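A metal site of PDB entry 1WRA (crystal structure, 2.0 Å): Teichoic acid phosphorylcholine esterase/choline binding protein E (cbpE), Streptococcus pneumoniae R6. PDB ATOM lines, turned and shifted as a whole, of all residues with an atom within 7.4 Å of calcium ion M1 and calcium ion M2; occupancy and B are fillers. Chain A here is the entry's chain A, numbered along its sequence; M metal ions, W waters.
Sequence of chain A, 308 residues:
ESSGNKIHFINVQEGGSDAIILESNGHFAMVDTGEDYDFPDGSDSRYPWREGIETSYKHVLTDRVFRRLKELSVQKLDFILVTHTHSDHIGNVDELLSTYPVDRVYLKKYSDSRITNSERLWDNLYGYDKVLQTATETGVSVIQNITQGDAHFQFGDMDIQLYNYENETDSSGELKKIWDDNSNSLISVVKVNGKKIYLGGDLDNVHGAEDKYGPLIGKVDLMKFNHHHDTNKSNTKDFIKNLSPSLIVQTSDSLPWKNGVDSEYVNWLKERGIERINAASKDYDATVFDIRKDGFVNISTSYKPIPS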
ATOM      1  N   THR A  33      20.894  26.904 -22.573  1.00  0.00           N
ATOM      2  CA  THR A  33      20.887  26.560 -21.122  1.00  0.00           C
ATOM      3  C   THR A  33      22.238  26.342 -20.516  1.00  0.00           C
ATOM      4  O   THR A  33      22.345  26.118 -19.313  1.00  0.00           O
ATOM      5  CB  THR A  33      20.047  25.295 -20.830  1.00  0.00           C
ATOM      6  OG1 THR A  33      20.646  24.125 -21.459  1.00  0.00           O
ATOM      7  CG2 THR A  33      18.673  25.437 -21.383  1.00  0.00           C
ATOM      8  N   GLY A  34      23.270  26.402 -21.341  1.00  0.00           N
ATOM      9  CA  GLY A  34      24.635  26.325 -20.867  1.00  0.00           C
ATOM     10  C   GLY A  34      25.130  24.918 -20.657  1.00  0.00           C
ATOM     11  O   GLY A  34      24.346  23.976 -20.654  1.00  0.00           O
ATOM     12  N   GLU A  35      26.445  24.802 -20.479  1.00  0.00           N
ATOM     13  CA  GLU A  35      27.146  23.567 -20.229  1.00  0.00           C
ATOM     14  C   GLU A  35      26.790  23.056 -18.818  1.00  0.00           C
ATOM     15  O   GLU A  35      26.610  23.867 -17.888  1.00  0.00           O
ATOM     16  CB  GLU A  35      28.663  23.818 -20.293  1.00  0.00           C
ATOM     17  CG  GLU A  35      29.533  22.584 -20.064  1.00  0.00           C
ATOM     18  CD  GLU A  35      29.296  21.535 -21.143  1.00  0.00           C
ATOM     19  OE1 GLU A  35      29.780  21.756 -22.293  1.00  0.00           O
ATOM     20  OE2 GLU A  35      28.546  20.555 -20.860  1.00  0.00           O
ATOM     21  N   ASP A  36      26.677  21.737 -18.685  1.00  0.00           N
ATOM     22  CA  ASP A  36      26.316  21.058 -17.447  1.00  0.00           C
ATOM     23  C   ASP A  36      27.437  20.160 -16.909  1.00  0.00           C
ATOM     24  O   ASP A  36      28.323  19.738 -17.663  1.00  0.00           O
ATOM     25  CB  ASP A  36      25.034  20.237 -17.669  1.00  0.00           C
ATOM     26  CG  ASP A  36      25.236  19.003 -18.552  1.00  0.00           C
ATOM     27  OD1 ASP A  36      26.065  19.034 -19.514  1.00  0.00           O
ATOM     28  OD2 ASP A  36      24.521  17.980 -18.371  1.00  0.00           O
ATOM     29  N   TYR A  37      27.396  19.853 -15.605  1.00  0.00           N
ATOM     30  CA  TYR A  37      28.354  18.931 -14.968  1.00  0.00           C
ATOM     31  C   TYR A  37      28.409  17.542 -15.618  1.00  0.00           C
ATOM     32  O   TYR A  37      29.485  16.970 -15.799  1.00  0.00           O
ATOM     33  CB  TYR A  37      28.032  18.744 -13.465  1.00  0.00           C
ATOM     34  CG  TYR A  37      28.270  19.994 -12.700  1.00  0.00           C
ATOM     35  CD1 TYR A  37      29.570  20.471 -12.527  1.00  0.00           C
ATOM     36  CD2 TYR A  37      27.231  20.729 -12.183  1.00  0.00           C
ATOM     37  CE1 TYR A  37      29.826  21.615 -11.827  1.00  0.00           C
ATOM     38  CE2 TYR A  37      27.492  21.920 -11.482  1.00  0.00           C
ATOM     39  CZ  TYR A  37      28.779  22.349 -11.322  1.00  0.00           C
ATOM     40  OH  TYR A  37      29.076  23.498 -10.644  1.00  0.00           O
ATOM     41  N   ASP A  38      27.250  17.030 -15.973  1.00  0.00           N
ATOM     42  CA  ASP A  38      27.151  15.649 -16.465  1.00  0.00           C
ATOM     43  C   ASP A  38      27.774  15.534 -17.879  1.00  0.00           C
ATOM     44  O   ASP A  38      27.944  16.531 -18.589  1.00  0.00           O
ATOM     45  CB  ASP A  38      25.656  15.256 -16.394  1.00  0.00           C
ATOM     46  CG  ASP A  38      25.379  13.811 -16.683  1.00  0.00           C
ATOM     47  OD1 ASP A  38      26.231  12.947 -16.425  1.00  0.00           O
ATOM     48  OD2 ASP A  38      24.290  13.465 -17.205  1.00  0.00           O
ATOM     49  N   PHE A  39      28.162  14.314 -18.230  1.00  0.00           N
ATOM     50  CA  PHE A  39      28.658  13.948 -19.549  1.00  0.00           C
ATOM     51  C   PHE A  39      28.726  12.434 -19.557  1.00  0.00           C
ATOM     52  O   PHE A  39      28.841  11.798 -18.505  1.00  0.00           O
ATOM     53  CB  PHE A  39      30.063  14.537 -19.830  1.00  0.00           C
ATOM     54  CG  PHE A  39      31.124  14.185 -18.815  1.00  0.00           C
ATOM     55  CD1 PHE A  39      31.899  13.039 -18.950  1.00  0.00           C
ATOM     56  CD2 PHE A  39      31.413  15.040 -17.746  1.00  0.00           C
ATOM     57  CE1 PHE A  39      32.903  12.744 -18.049  1.00  0.00           C
ATOM     58  CE2 PHE A  39      32.422  14.737 -16.849  1.00  0.00           C
ATOM     59  CZ  PHE A  39      33.179  13.577 -17.012  1.00  0.00           C
ATOM     60  N   PRO A  40      28.665  11.831 -20.726  1.00  0.00           N
ATOM     61  CA  PRO A  40      28.769  10.367 -20.768  1.00  0.00           C
ATOM     62  C   PRO A  40      30.228   9.923 -20.628  1.00  0.00           C
ATOM     63  O   PRO A  40      31.131  10.562 -21.168  1.00  0.00           O
ATOM     64  CB  PRO A  40      28.248  10.042 -22.153  1.00  0.00           C
ATOM     65  CG  PRO A  40      28.652  11.271 -23.018  1.00  0.00           C
ATOM     66  CD  PRO A  40      28.499  12.433 -22.084  1.00  0.00           C
ATOM     67  N   ILE A  53      34.920  15.600 -25.617  1.00  0.00           N
ATOM     68  CA  ILE A  53      33.720  15.723 -24.791  1.00  0.00           C
ATOM     69  C   ILE A  53      34.089  16.584 -23.578  1.00  0.00           C
ATOM     70  O   ILE A  53      35.065  16.360 -22.931  1.00  0.00           O
ATOM     71  CB  ILE A  53      33.209  14.349 -24.327  1.00  0.00           C
ATOM     72  CG1 ILE A  53      32.526  13.616 -25.513  1.00  0.00           C
ATOM     73  CG2 ILE A  53      32.269  14.506 -23.097  1.00  0.00           C
ATOM     74  CD1 ILE A  53      31.964  12.225 -25.177  1.00  0.00           C
ATOM     75  N   GLU A  54      33.272  17.559 -23.279  1.00  0.00           N
ATOM     76  CA  GLU A  54      33.580  18.425 -22.173  1.00  0.00           C
ATOM     77  C   GLU A  54      33.332  17.902 -20.752  1.00  0.00           C
ATOM     78  O   GLU A  54      32.324  17.247 -20.504  1.00  0.00           O
ATOM     79  CB  GLU A  54      32.697  19.676 -22.270  1.00  0.00           C
ATOM     80  CG  GLU A  54      32.874  20.698 -21.133  1.00  0.00           C
ATOM     81  CD  GLU A  54      34.218  21.359 -21.252  1.00  0.00           C
ATOM     82  OE1 GLU A  54      35.176  20.959 -20.546  1.00  0.00           O
ATOM     83  OE2 GLU A  54      34.329  22.223 -22.126  1.00  0.00           O
ATOM     84  N   THR A  55      34.272  18.144 -19.859  1.00  0.00           N
ATOM     85  CA  THR A  55      34.489  17.391 -18.613  1.00  0.00           C
ATOM     86  C   THR A  55      34.811  18.502 -17.542  1.00  0.00           C
ATOM     87  O   THR A  55      34.592  18.315 -16.347  1.00  0.00           O
ATOM     88  CB  THR A  55      35.541  16.277 -18.604  1.00  0.00           C
ATOM     89  OG1 THR A  55      36.851  16.836 -18.749  1.00  0.00           O
ATOM     90  CG2 THR A  55      35.287  15.273 -19.738  1.00  0.00           C
ATOM     91  N   SER A  56      35.311  19.670 -17.985  1.00  0.00           N
ATOM     92  CA  SER A  56      35.815  20.669 -17.047  1.00  0.00           C
ATOM     93  C   SER A  56      34.744  21.500 -16.313  1.00  0.00           C
ATOM     94  O   SER A  56      33.924  22.203 -16.933  1.00  0.00           O
ATOM     95  CB  SER A  56      36.830  21.581 -17.727  1.00  0.00           C
ATOM     96  OG  SER A  56      37.266  22.607 -16.839  1.00  0.00           O
ATOM     97  N   VAL A  60      31.410  24.862 -16.848  1.00  0.00           N
ATOM     98  CA  VAL A  60      30.031  24.542 -16.490  1.00  0.00           C
ATOM     99  C   VAL A  60      29.253  25.782 -16.061  1.00  0.00           C
ATOM    100  O   VAL A  60      29.735  26.571 -15.272  1.00  0.00           O
ATOM    101  CB  VAL A  60      29.988  23.447 -15.376  1.00  0.00           C
ATOM    102  CG1 VAL A  60      28.614  23.298 -14.800  1.00  0.00           C
ATOM    103  CG2 VAL A  60      30.436  22.128 -15.948  1.00  0.00           C
ATOM    104  N   THR A  62      25.831  25.455 -15.038  1.00  0.00           N
ATOM    105  CA  THR A  62      24.736  24.966 -14.210  1.00  0.00           C
ATOM    106  C   THR A  62      24.434  25.837 -13.009  1.00  0.00           C
ATOM    107  O   THR A  62      23.292  26.233 -12.823  1.00  0.00           O
ATOM    108  CB  THR A  62      25.028  23.541 -13.740  1.00  0.00           C
ATOM    109  OG1 THR A  62      25.248  22.706 -14.874  1.00  0.00           O
ATOM    110  CG2 THR A  62      23.796  22.939 -13.028  1.00  0.00           C
ATOM    111  N   SER A  87      26.833  20.348 -26.020  1.00  0.00           N
ATOM    112  CA  SER A  87      26.654  20.299 -24.568  1.00  0.00           C
ATOM    113  C   SER A  87      26.665  21.680 -23.903  1.00  0.00           C
ATOM    114  O   SER A  87      25.952  21.912 -22.896  1.00  0.00           O
ATOM    115  CB  SER A  87      27.756  19.419 -23.964  1.00  0.00           C
ATOM    116  OG  SER A  87      29.074  19.956 -24.210  1.00  0.00           O
ATOM    117  N   ASP A  88      27.451  22.601 -24.465  1.00  0.00           N
ATOM    118  CA  ASP A  88      27.546  23.975 -23.942  1.00  0.00           C
ATOM    119  C   ASP A  88      26.328  24.863 -24.301  1.00  0.00           C
ATOM    120  O   ASP A  88      26.291  26.071 -23.999  1.00  0.00           O
ATOM    121  CB  ASP A  88      28.885  24.627 -24.367  1.00  0.00           C
ATOM    122  CG  ASP A  88      29.041  24.733 -25.879  1.00  0.00           C
ATOM    123  OD1 ASP A  88      29.050  23.674 -26.575  1.00  0.00           O
ATOM    124  OD2 ASP A  88      29.131  25.849 -26.436  1.00  0.00           O
ATOM    125  N   ILE A  90      22.822  22.779 -24.887  1.00  0.00           N
ATOM    126  CA  ILE A  90      21.710  21.905 -24.484  1.00  0.00           C
ATOM    127  C   ILE A  90      21.919  21.331 -23.082  1.00  0.00           C
ATOM    128  O   ILE A  90      21.027  20.714 -22.509  1.00  0.00           O
ATOM    129  CB  ILE A  90      21.578  20.770 -25.501  1.00  0.00           C
ATOM    130  CG1 ILE A  90      20.151  20.211 -25.516  1.00  0.00           C
ATOM    131  CG2 ILE A  90      22.608  19.640 -25.207  1.00  0.00           C
ATOM    132  CD1 ILE A  90      19.912  19.258 -26.693  1.00  0.00           C
ATOM    133  N   GLY A  91      23.100  21.569 -22.530  1.00  0.00           N
ATOM    134  CA  GLY A  91      23.532  20.872 -21.336  1.00  0.00           C
ATOM    135  C   GLY A  91      22.578  20.858 -20.157  1.00  0.00           C
ATOM    136  O   GLY A  91      22.410  19.804 -19.576  1.00  0.00           O
ATOM    137  N   ASN A  92      21.992  21.988 -19.772  1.00  0.00           N
ATOM    138  CA  ASN A  92      21.145  22.031 -18.582  1.00  0.00           C
ATOM    139  C   ASN A  92      19.640  21.826 -18.842  1.00  0.00           C
ATOM    140  O   ASN A  92      18.799  22.059 -17.960  1.00  0.00           O
ATOM    141  CB  ASN A  92      21.381  23.305 -17.783  1.00  0.00           C
ATOM    142  CG  ASN A  92      22.747  23.319 -17.106  1.00  0.00           C
ATOM    143  OD1 ASN A  92      23.033  22.519 -16.190  1.00  0.00           O
ATOM    144  ND2 ASN A  92      23.610  24.246 -17.557  1.00  0.00           N
ATOM    145  N   VAL A  93      19.282  21.371 -20.043  1.00  0.00           N
ATOM    146  CA  VAL A  93      17.861  21.258 -20.340  1.00  0.00           C
ATOM    147  C   VAL A  93      17.142  20.233 -19.455  1.00  0.00           C
ATOM    148  O   VAL A  93      16.055  20.538 -18.937  1.00  0.00           O
ATOM    149  CB  VAL A  93      17.586  20.919 -21.802  1.00  0.00           C
ATOM    150  CG1 VAL A  93      16.093  20.652 -22.037  1.00  0.00           C
ATOM    151  CG2 VAL A  93      17.998  22.092 -22.685  1.00  0.00           C
ATOM    152  N   ASP A  94      17.681  19.018 -19.342  1.00  0.00           N
ATOM    153  CA  ASP A  94      17.026  17.983 -18.521  1.00  0.00           C
ATOM    154  C   ASP A  94      16.993  18.343 -17.009  1.00  0.00           C
ATOM    155  O   ASP A  94      16.038  18.033 -16.313  1.00  0.00           O
ATOM    156  CB  ASP A  94      17.648  16.586 -18.728  1.00  0.00           C
ATOM    157  CG  ASP A  94      19.149  16.547 -18.422  1.00  0.00           C
ATOM    158  OD1 ASP A  94      19.933  17.299 -19.044  1.00  0.00           O
ATOM    159  OD2 ASP A  94      19.657  15.790 -17.598  1.00  0.00           O
ATOM    160  N   GLU A  95      18.036  19.002 -16.529  1.00  0.00           N
ATOM    161  CA  GLU A  95      18.020  19.539 -15.154  1.00  0.00           C
ATOM    162  C   GLU A  95      16.918  20.576 -14.975  1.00  0.00           C
ATOM    163  O   GLU A  95      16.270  20.627 -13.927  1.00  0.00           O
ATOM    164  CB  GLU A  95      19.378  20.142 -14.754  1.00  0.00           C
ATOM    165  CG  GLU A  95      20.527  19.128 -14.588  1.00  0.00           C
ATOM    166  CD  GLU A  95      21.219  18.740 -15.919  1.00  0.00           C
ATOM    167  OE1 GLU A  95      20.892  19.272 -16.988  1.00  0.00           O
ATOM    168  OE2 GLU A  95      22.085  17.856 -15.918  1.00  0.00           O
ATOM    169  N   LEU A  96      16.707  21.432 -15.979  1.00  0.00           N
ATOM    170  CA  LEU A  96      15.663  22.448 -15.904  1.00  0.00           C
ATOM    171  C   LEU A  96      14.298  21.761 -15.953  1.00  0.00           C
ATOM    172  O   LEU A  96      13.401  22.121 -15.184  1.00  0.00           O
ATOM    173  CB  LEU A  96      15.798  23.495 -17.046  1.00  0.00           C
ATOM    174  CG  LEU A  96      16.963  24.478 -16.860  1.00  0.00           C
ATOM    175  CD1 LEU A  96      17.397  25.245 -18.170  1.00  0.00           C
ATOM    176  CD2 LEU A  96      16.688  25.508 -15.749  1.00  0.00           C
ATOM    177  N   ASP A 123      29.322  14.403 -27.528  1.00  0.00           N
ATOM    178  CA  ASP A 123      28.344  14.399 -26.510  1.00  0.00           C
ATOM    179  C   ASP A 123      26.915  14.674 -27.028  1.00  0.00           C
ATOM    180  O   ASP A 123      25.932  14.751 -26.271  1.00  0.00           O
ATOM    181  CB  ASP A 123      28.760  15.690 -25.589  1.00  0.00           C
ATOM    182  CG  ASP A 123      28.619  15.314 -24.292  1.00  0.00           C
ATOM    183  OD1 ASP A 123      28.380  14.060 -24.399  1.00  0.00           O
ATOM    184  OD2 ASP A 123      28.570  15.941 -23.238  1.00  0.00           O
ATOM    185  N   TYR A 126      23.808  12.285 -26.479  1.00  0.00           N
ATOM    186  CA  TYR A 126      23.516  12.128 -25.064  1.00  0.00           C
ATOM    187  C   TYR A 126      22.644  13.302 -24.584  1.00  0.00           C
ATOM    188  O   TYR A 126      21.602  13.114 -23.934  1.00  0.00           O
ATOM    189  CB  TYR A 126      24.819  12.047 -24.286  1.00  0.00           C
ATOM    190  CG  TYR A 126      24.658  11.838 -22.803  1.00  0.00           C
ATOM    191  CD1 TYR A 126      24.872  12.857 -21.916  1.00  0.00           C
ATOM    192  CD2 TYR A 126      24.318  10.579 -22.303  1.00  0.00           C
ATOM    193  CE1 TYR A 126      24.712  12.658 -20.552  1.00  0.00           C
ATOM    194  CE2 TYR A 126      24.171  10.366 -20.946  1.00  0.00           C
ATOM    195  CZ  TYR A 126      24.380  11.418 -20.076  1.00  0.00           C
ATOM    196  OH  TYR A 126      24.276  11.213 -18.718  1.00  0.00           O
ATOM    197  N   GLY A 127      23.051  14.509 -24.935  1.00  0.00           N
ATOM    198  CA  GLY A 127      22.278  15.701 -24.621  1.00  0.00           C
ATOM    199  C   GLY A 127      20.884  15.792 -25.243  1.00  0.00           C
ATOM    200  O   GLY A 127      19.932  16.120 -24.554  1.00  0.00           O
ATOM    201  N   LYS A 130      18.669  13.152 -23.608  1.00  0.00           N
ATOM    202  CA  LYS A 130      18.266  13.673 -22.296  1.00  0.00           C
ATOM    203  C   LYS A 130      17.069  14.616 -22.382  1.00  0.00           C
ATOM    204  O   LYS A 130      16.187  14.597 -21.524  1.00  0.00           O
ATOM    205  CB  LYS A 130      19.426  14.386 -21.573  1.00  0.00           C
ATOM    206  CG  LYS A 130      20.421  13.432 -20.898  1.00  0.00           C
ATOM    207  CD  LYS A 130      19.858  12.881 -19.585  1.00  0.00           C
ATOM    208  CE  LYS A 130      20.788  11.846 -18.969  1.00  0.00           C
ATOM    209  NZ  LYS A 130      20.229  11.265 -17.726  1.00  0.00           N
HETATM  210 CA    CA M   1      22.222  17.683 -18.495  1.00  0.00          CA
HETATM  211 CA    CA M   2      28.341  18.444 -19.875  1.00  0.00          CA
HETATM  212  O   HOH W   1      30.502  18.582 -19.027  1.00  0.00           O
HETATM  213  O   HOH W   2      22.380  15.319 -18.094  1.00  0.00           O
HETATM  214  O   HOH W   3      29.776  17.481 -21.491  1.00  0.00           O
HETATM  215  O   HOH W   4      27.020  17.032 -21.541  1.00  0.00           O
HETATM  216  O   HOH W   5      22.472  17.070 -20.952  1.00  0.00           O
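O of Gly 34 lies close to N of Gly 91, at 3.3 Å. The backbone carbonyl oxygen (O) of Glu 35 is in hydrogen-bond range of the backbone NH (N) of Thr 62, 3.4 Å away. The side-chain hydroxyl of Ser 87 is in hydrogen-bond range of the side-chain carboxylate of Glu 35, 2.7 Å away. OD2 of Asp 38 is in hydrogen-bond range of OH of Tyr 126 (2.7 Å). N of Asp 88 lies within hydrogen-bond range of OE1 of Glu 35 (3.3 Å). The backbone carbonyl oxygen (O) of Glu 35 is in hydrogen-bond range of the side-chain amide nitrogen (ND2) of Asn 92 (3.0 Å).
Calcium ion M1 is bound by OD2 of Asp 36 (2.3 Å), OD1 of Asp 94 (2.4 Å), O of Gly 91 (2.4 Å), water W2 (2.4 Å), water W5 (2.5 Å), OE1 of Glu 95 (2.6 Å) and OE2 of Glu 95 (2.6 Å). Calcium ion M1 has seven donor atoms within binding distance.
Calcium ion M2 is bound by water W1, O of Asp 38, OE2 of Glu 35, water W3, OD1 of Asp 36, water W4 and O of Asp 36. Calcium ion M2 has seven donor atoms within binding distance.
Water W2 lies within hydrogen-bond range of the side-chain carboxylate (OD2) of Asp 38 (2.8 Å) and the side-chain carboxylate (OD2) of Asp 94 (2.8 Å). Water W3 lies within hydrogen-bond range of OD2 of Asp 123 (2.6 Å) and O of Glu 54 (2.7 Å).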
